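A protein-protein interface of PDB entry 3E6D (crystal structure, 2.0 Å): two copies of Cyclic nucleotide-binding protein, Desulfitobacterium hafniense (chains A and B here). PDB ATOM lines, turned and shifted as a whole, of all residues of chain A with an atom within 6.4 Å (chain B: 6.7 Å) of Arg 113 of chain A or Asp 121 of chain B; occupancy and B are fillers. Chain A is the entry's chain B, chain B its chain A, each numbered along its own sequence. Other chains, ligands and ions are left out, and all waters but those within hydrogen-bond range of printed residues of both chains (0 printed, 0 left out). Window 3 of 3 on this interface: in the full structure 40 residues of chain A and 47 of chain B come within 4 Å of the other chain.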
ATOM      1  N   SER A 108      37.547 -22.605   5.827  1.00  0.00           N
ATOM      2  CA  SER A 108      37.595 -22.025   7.166  1.00  0.00           C
ATOM      3  C   SER A 108      36.497 -22.633   8.035  1.00  0.00           C
ATOM      4  O   SER A 108      35.654 -23.382   7.540  1.00  0.00           O
ATOM      5  CB  SER A 108      37.396 -20.515   7.101  1.00  0.00           C
ATOM      6  OG  SER A 108      36.088 -20.208   6.657  1.00  0.00           O
ATOM      7  N   GLU A 109      36.494 -22.306   9.325  1.00  0.00           N
ATOM      8  CA  GLU A 109      35.440 -22.793  10.212  1.00  0.00           C
ATOM      9  C   GLU A 109      34.096 -22.205   9.800  1.00  0.00           C
ATOM     10  O   GLU A 109      33.068 -22.887   9.838  1.00  0.00           O
ATOM     11  CB  GLU A 109      35.739 -22.468  11.681  1.00  0.00           C
ATOM     12  CG  GLU A 109      34.653 -22.934  12.642  1.00  0.00           C
ATOM     13  CD  GLU A 109      34.785 -22.321  14.026  1.00  0.00           C
ATOM     14  OE1 GLU A 109      35.688 -22.729  14.783  1.00  0.00           O
ATOM     15  OE2 GLU A 109      33.975 -21.431  14.359  1.00  0.00           O
ATOM     16  N   LYS A 110      34.104 -20.941   9.397  1.00  0.00           N
ATOM     17  CA  LYS A 110      32.882 -20.297   8.933  1.00  0.00           C
ATOM     18  C   LYS A 110      32.287 -21.004   7.709  1.00  0.00           C
ATOM     19  O   LYS A 110      31.085 -21.254   7.654  1.00  0.00           O
ATOM     20  CB  LYS A 110      33.122 -18.818   8.623  1.00  0.00           C
ATOM     21  CG  LYS A 110      31.873 -18.104   8.135  1.00  0.00           C
ATOM     22  CD  LYS A 110      30.709 -18.365   9.084  1.00  0.00           C
ATOM     23  CE  LYS A 110      29.366 -18.277   8.370  1.00  0.00           C
ATOM     24  NZ  LYS A 110      28.237 -18.659   9.264  1.00  0.00           N
ATOM     25  N   SER A 111      33.125 -21.329   6.730  1.00  0.00           N
ATOM     26  CA  SER A 111      32.622 -21.991   5.528  1.00  0.00           C
ATOM     27  C   SER A 111      32.135 -23.412   5.818  1.00  0.00           C
ATOM     28  O   SER A 111      31.214 -23.900   5.163  1.00  0.00           O
ATOM     29  CB  SER A 111      33.657 -21.993   4.404  1.00  0.00           C
ATOM     30  OG  SER A 111      34.719 -22.859   4.698  1.00  0.00           O
ATOM     31  N   LEU A 112      32.735 -24.074   6.806  1.00  0.00           N
ATOM     32  CA  LEU A 112      32.254 -25.398   7.205  1.00  0.00           C
ATOM     33  C   LEU A 112      30.874 -25.339   7.856  1.00  0.00           C
ATOM     34  O   LEU A 112      30.057 -26.238   7.663  1.00  0.00           O
ATOM     35  CB  LEU A 112      33.253 -26.107   8.120  1.00  0.00           C
ATOM     36  CG  LEU A 112      34.528 -26.596   7.436  1.00  0.00           C
ATOM     37  CD1 LEU A 112      35.445 -27.307   8.423  1.00  0.00           C
ATOM     38  CD2 LEU A 112      34.178 -27.513   6.272  1.00  0.00           C
ATOM     39  N   ARG A 113      30.614 -24.288   8.631  1.00  0.00           N
ATOM     40  CA  ARG A 113      29.279 -24.096   9.189  1.00  0.00           C
ATOM     41  C   ARG A 113      28.267 -23.973   8.057  1.00  0.00           C
ATOM     42  O   ARG A 113      27.171 -24.527   8.118  1.00  0.00           O
ATOM     43  CB  ARG A 113      29.211 -22.849  10.076  1.00  0.00           C
ATOM     44  CG  ARG A 113      29.966 -22.957  11.384  1.00  0.00           C
ATOM     45  CD  ARG A 113      29.781 -21.704  12.233  1.00  0.00           C
ATOM     46  NE  ARG A 113      30.638 -21.722  13.414  1.00  0.00           N
ATOM     47  CZ  ARG A 113      30.243 -22.105  14.624  1.00  0.00           C
ATOM     48  NH1 ARG A 113      28.994 -22.503  14.833  1.00  0.00           N
ATOM     49  NH2 ARG A 113      31.103 -22.088  15.631  1.00  0.00           N
ATOM     50  N   THR A 114      28.642 -23.231   7.022  1.00  0.00           N
ATOM     51  CA  THR A 114      27.787 -23.062   5.860  1.00  0.00           C
ATOM     52  C   THR A 114      27.552 -24.412   5.188  1.00  0.00           C
ATOM     53  O   THR A 114      26.421 -24.748   4.839  1.00  0.00           O
ATOM     54  CB  THR A 114      28.405 -22.078   4.857  1.00  0.00           C
ATOM     55  OG1 THR A 114      28.717 -20.855   5.535  1.00  0.00           O
ATOM     56  CG2 THR A 114      27.441 -21.798   3.711  1.00  0.00           C
ATOM     57  N   VAL A 115      28.618 -25.187   5.022  1.00  0.00           N
ATOM     58  CA  VAL A 115      28.480 -26.529   4.453  1.00  0.00           C
ATOM     59  C   VAL A 115      27.503 -27.366   5.273  1.00  0.00           C
ATOM     60  O   VAL A 115      26.568 -27.954   4.731  1.00  0.00           O
ATOM     61  CB  VAL A 115      29.824 -27.278   4.383  1.00  0.00           C
ATOM     62  CG1 VAL A 115      29.577 -28.773   4.112  1.00  0.00           C
ATOM     63  CG2 VAL A 115      30.730 -26.667   3.316  1.00  0.00           C
ATOM     64  N   PHE A 116      27.722 -27.407   6.585  1.00  0.00           N
ATOM     65  CA  PHE A 116      26.914 -28.241   7.471  1.00  0.00           C
ATOM     66  C   PHE A 116      25.437 -27.839   7.498  1.00  0.00           C
ATOM     67  O   PHE A 116      24.556 -28.692   7.603  1.00  0.00           O
ATOM     68  CB  PHE A 116      27.492 -28.256   8.891  1.00  0.00           C
ATOM     69  CG  PHE A 116      28.892 -28.806   8.976  1.00  0.00           C
ATOM     70  CD1 PHE A 116      29.337 -29.763   8.072  1.00  0.00           C
ATOM     71  CD2 PHE A 116      29.760 -28.379   9.975  1.00  0.00           C
ATOM     72  CE1 PHE A 116      30.616 -30.278   8.157  1.00  0.00           C
ATOM     73  CE2 PHE A 116      31.039 -28.884  10.063  1.00  0.00           C
ATOM     74  CZ  PHE A 116      31.473 -29.838   9.149  1.00  0.00           C
ATOM     75  N   ARG A 117      25.171 -26.540   7.403  1.00  0.00           N
ATOM     76  CA  ARG A 117      23.799 -26.037   7.405  1.00  0.00           C
ATOM     77  C   ARG A 117      23.055 -26.419   6.129  1.00  0.00           C
ATOM     78  O   ARG A 117      21.824 -26.488   6.113  1.00  0.00           O
ATOM     79  CB  ARG A 117      23.776 -24.516   7.604  1.00  0.00           C
ATOM     80  CG  ARG A 117      24.413 -24.086   8.912  1.00  0.00           C
ATOM     81  CD  ARG A 117      24.319 -22.590   9.160  1.00  0.00           C
ATOM     82  NE  ARG A 117      24.976 -22.230  10.416  1.00  0.00           N
ATOM     83  CZ  ARG A 117      24.981 -21.006  10.937  1.00  0.00           C
ATOM     84  NH1 ARG A 117      24.359 -20.012  10.315  1.00  0.00           N
ATOM     85  NH2 ARG A 117      25.605 -20.778  12.085  1.00  0.00           N
ATOM     86  N   THR A 118      23.805 -26.661   5.059  1.00  0.00           N
ATOM     87  CA  THR A 118      23.224 -27.151   3.814  1.00  0.00           C
ATOM     88  C   THR A 118      23.011 -28.665   3.829  1.00  0.00           C
ATOM     89  O   THR A 118      22.060 -29.172   3.235  1.00  0.00           O
ATOM     90  CB  THR A 118      24.100 -26.762   2.598  1.00  0.00           C
ATOM     91  OG1 THR A 118      24.113 -25.333   2.464  1.00  0.00           O
ATOM     92  CG2 THR A 118      23.555 -27.380   1.325  1.00  0.00           C
ATOM     93  N   PHE B 116      23.974 -31.444  18.181  1.00  0.00           N
ATOM     94  CA  PHE B 116      24.417 -30.447  17.206  1.00  0.00           C
ATOM     95  C   PHE B 116      23.315 -29.464  16.826  1.00  0.00           C
ATOM     96  O   PHE B 116      23.586 -28.300  16.555  1.00  0.00           O
ATOM     97  CB  PHE B 116      24.992 -31.116  15.941  1.00  0.00           C
ATOM     98  CG  PHE B 116      26.159 -32.025  16.208  1.00  0.00           C
ATOM     99  CD1 PHE B 116      27.030 -31.765  17.254  1.00  0.00           C
ATOM    100  CD2 PHE B 116      26.390 -33.138  15.406  1.00  0.00           C
ATOM    101  CE1 PHE B 116      28.102 -32.603  17.510  1.00  0.00           C
ATOM    102  CE2 PHE B 116      27.464 -33.978  15.652  1.00  0.00           C
ATOM    103  CZ  PHE B 116      28.318 -33.713  16.705  1.00  0.00           C
ATOM    104  N   THR B 118      21.079 -28.369  18.803  1.00  0.00           N
ATOM    105  CA  THR B 118      20.935 -27.444  19.920  1.00  0.00           C
ATOM    106  C   THR B 118      22.107 -26.474  19.998  1.00  0.00           C
ATOM    107  O   THR B 118      21.920 -25.273  20.213  1.00  0.00           O
ATOM    108  CB  THR B 118      20.835 -28.204  21.260  1.00  0.00           C
ATOM    109  OG1 THR B 118      19.774 -29.166  21.190  1.00  0.00           O
ATOM    110  CG2 THR B 118      20.562 -27.228  22.408  1.00  0.00           C
ATOM    111  N   ASP B 119      23.314 -27.008  19.831  1.00  0.00           N
ATOM    112  CA  ASP B 119      24.537 -26.222  19.964  1.00  0.00           C
ATOM    113  C   ASP B 119      25.523 -26.554  18.843  1.00  0.00           C
ATOM    114  O   ASP B 119      26.369 -27.445  18.976  1.00  0.00           O
ATOM    115  CB  ASP B 119      25.181 -26.478  21.327  1.00  0.00           C
ATOM    116  CG  ASP B 119      26.383 -25.592  21.584  1.00  0.00           C
ATOM    117  OD1 ASP B 119      26.638 -24.679  20.778  1.00  0.00           O
ATOM    118  OD2 ASP B 119      27.072 -25.804  22.602  1.00  0.00           O
ATOM    119  N   GLU B 120      25.413 -25.820  17.745  1.00  0.00           N
ATOM    120  CA  GLU B 120      26.266 -26.032  16.579  1.00  0.00           C
ATOM    121  C   GLU B 120      27.746 -26.081  16.946  1.00  0.00           C
ATOM    122  O   GLU B 120      28.534 -26.770  16.293  1.00  0.00           O
ATOM    123  CB  GLU B 120      26.017 -24.935  15.542  1.00  0.00           C
ATOM    124  CG  GLU B 120      26.552 -25.246  14.155  1.00  0.00           C
ATOM    125  CD  GLU B 120      26.337 -24.098  13.180  1.00  0.00           C
ATOM    126  OE1 GLU B 120      26.884 -22.999  13.418  1.00  0.00           O
ATOM    127  OE2 GLU B 120      25.624 -24.295  12.174  1.00  0.00           O
ATOM    128  N   ASP B 121      28.124 -25.360  17.998  1.00  0.00           N
ATOM    129  CA  ASP B 121      29.535 -25.261  18.379  1.00  0.00           C
ATOM    130  C   ASP B 121      30.153 -26.599  18.791  1.00  0.00           C
ATOM    131  O   ASP B 121      31.356 -26.807  18.627  1.00  0.00           O
ATOM    132  CB  ASP B 121      29.730 -24.229  19.498  1.00  0.00           C
ATOM    133  CG  ASP B 121      29.493 -22.806  19.025  1.00  0.00           C
ATOM    134  OD1 ASP B 121      29.378 -22.591  17.799  1.00  0.00           O
ATOM    135  OD2 ASP B 121      29.422 -21.902  19.881  1.00  0.00           O
ATOM    136  N   MET B 122      29.330 -27.499  19.326  1.00  0.00           N
ATOM    137  CA  MET B 122      29.809 -28.810  19.767  1.00  0.00           C
ATOM    138  C   MET B 122      30.429 -29.618  18.626  1.00  0.00           C
ATOM    139  O   MET B 122      31.333 -30.426  18.854  1.00  0.00           O
ATOM    140  CB  MET B 122      28.683 -29.621  20.419  1.00  0.00           C
ATOM    141  CG  MET B 122      28.323 -29.194  21.844  1.00  0.00           C
ATOM    142  SD  MET B 122      29.738 -29.200  22.956  1.00  0.00           S
ATOM    143  CE  MET B 122      30.194 -27.471  22.874  1.00  0.00           C
ATOM    144  N   ILE B 123      29.925 -29.419  17.411  1.00  0.00           N
ATOM    145  CA  ILE B 123      30.520 -30.034  16.229  1.00  0.00           C
ATOM    146  C   ILE B 123      32.020 -29.790  16.229  1.00  0.00           C
ATOM    147  O   ILE B 123      32.825 -30.709  16.061  1.00  0.00           O
ATOM    148  CB  ILE B 123      29.965 -29.416  14.926  1.00  0.00           C
ATOM    149  CG1 ILE B 123      28.462 -29.669  14.791  1.00  0.00           C
ATOM    150  CG2 ILE B 123      30.726 -29.951  13.706  1.00  0.00           C
ATOM    151  CD1 ILE B 123      27.863 -28.992  13.584  1.00  0.00           C
ATOM    152  N   PHE B 124      32.390 -28.534  16.423  1.00  0.00           N
ATOM    153  CA  PHE B 124      33.788 -28.146  16.328  1.00  0.00           C
ATOM    154  C   PHE B 124      34.613 -28.525  17.557  1.00  0.00           C
ATOM    155  O   PHE B 124      35.831 -28.687  17.454  1.00  0.00           O
ATOM    156  CB  PHE B 124      33.900 -26.659  15.980  1.00  0.00           C
ATOM    157  CG  PHE B 124      33.265 -26.314  14.661  1.00  0.00           C
ATOM    158  CD1 PHE B 124      31.986 -25.784  14.606  1.00  0.00           C
ATOM    159  CD2 PHE B 124      33.938 -26.554  13.474  1.00  0.00           C
ATOM    160  CE1 PHE B 124      31.397 -25.484  13.390  1.00  0.00           C
ATOM    161  CE2 PHE B 124      33.358 -26.256  12.258  1.00  0.00           C
ATOM    162  CZ  PHE B 124      32.087 -25.718  12.213  1.00  0.00           C
ATOM    163  N   GLU B 125      33.952 -28.684  18.704  1.00  0.00           N
ATOM    164  CA  GLU B 125      34.604 -29.209  19.905  1.00  0.00           C
ATOM    165  C   GLU B 125      35.054 -30.637  19.647  1.00  0.00           C
ATOM    166  O   GLU B 125      36.193 -31.008  19.932  1.00  0.00           O
ATOM    167  CB  GLU B 125      33.647 -29.200  21.105  1.00  0.00           C
ATOM    168  CG  GLU B 125      33.329 -27.827  21.662  1.00  0.00           C
ATOM    169  CD  GLU B 125      34.504 -27.207  22.390  1.00  0.00           C
ATOM    170  OE1 GLU B 125      34.598 -25.959  22.413  1.00  0.00           O
ATOM    171  OE2 GLU B 125      35.339 -27.970  22.927  1.00  0.00           O
ATOM    172  N   ILE B 126      34.143 -31.444  19.112  1.00  0.00           N
ATOM    173  CA  ILE B 126      34.469 -32.824  18.761  1.00  0.00           C
ATOM    174  C   ILE B 126      35.535 -32.876  17.667  1.00  0.00           C
ATOM    175  O   ILE B 126      36.480 -33.656  17.745  1.00  0.00           O
ATOM    176  CB  ILE B 126      33.223 -33.608  18.326  1.00  0.00           C
ATOM    177  CG1 ILE B 126      32.329 -33.891  19.538  1.00  0.00           C
ATOM    178  CG2 ILE B 126      33.618 -34.919  17.659  1.00  0.00           C
ATOM    179  CD1 ILE B 126      31.056 -34.625  19.200  1.00  0.00           C
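NH1 of Arg 113 of chain A is in salt-bridge range of OE1 of Glu 120 of chain B. The side-chain carboxylate (OE2) of Glu 120 of chain B is in salt-bridge range of the guanidinium group (NE) of Arg 117 of chain A (2.8 Å). The side-chain carboxylate of Asp 121 of chain B is in salt-bridge range of the guanidinium group of Arg 113 of chain A, 2.8 Å away.
OD1 of Asp 119 of chain B sits close to N of Asp 121 of chain B, at 3.2 Å. The side-chain carboxylate (OE2) of Glu 109 of chain A is in salt-bridge range of the guanidinium group (NH2) of Arg 113 of chain A (3.2 Å).
CE2 of Phe 124 of chain B touches CG of Glu 109 of chain A, 3.6 Å away. Phe 124 of chain B touches Arg 113 of chain A (CE1 to CG, 3.5 Å). Ile 123 of chain B touches Phe 116 of chain A (CG2 to CE2, 3.8 Å). CZ of Phe 124 of chain B touches CE2 of Phe 116 of chain A, 3.97 Å away.
Of the printed residues of chain B, Glu 109 of chain A touches Phe 124. Printed residues of chain B within 4 Å of Arg 113 of chain A: Glu 120, Asp 121 and Phe 124. Printed residues of chain B within 4 Å of Arg 117 of chain A: Glu 120. Of chain A, only Arg 113 comes within 4 Å of Asp 121 of chain B. Of the printed residues of chain A, Phe 124 of chain B touches Glu 109 (3.6 Å), Arg 113 (3.5 Å) and Phe 116 (3.97 Å). The nearest residue of chain A that does not touch Asp 121 of chain B is Glu 109 of chain A (5.9 Å).
Printed residues of chain A that touch a printed residue of chain B: Glu 109, Arg 113, Phe 116 and Arg 117. Hydrophobic or aromatic side chains of chain A within 4 Å of the printed part of chain B: Phe 116. Of the 10 printed residues of chain B, 4 touch a printed residue of chain A. Hydrophobic or aromatic side chains of chain B within 4 Å of the printed part of chain A: Ile 123 and Phe 124. Among the printed residues, Asp or Glu carboxylates within 4 Å of a Lys or Arg side-chain nitrogen of the other chain: Arg 113 of chain A with Glu 120 of chain B, Arg 113 of chain A with Asp 121 of chain B and Arg 117 of chain A with Glu 120 of chain B.
Positions printed for both chains: 116 and 118. Of the 7 pairs that touch across the chains among the printed residues, none has its exchanged pair printed and touching as well.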
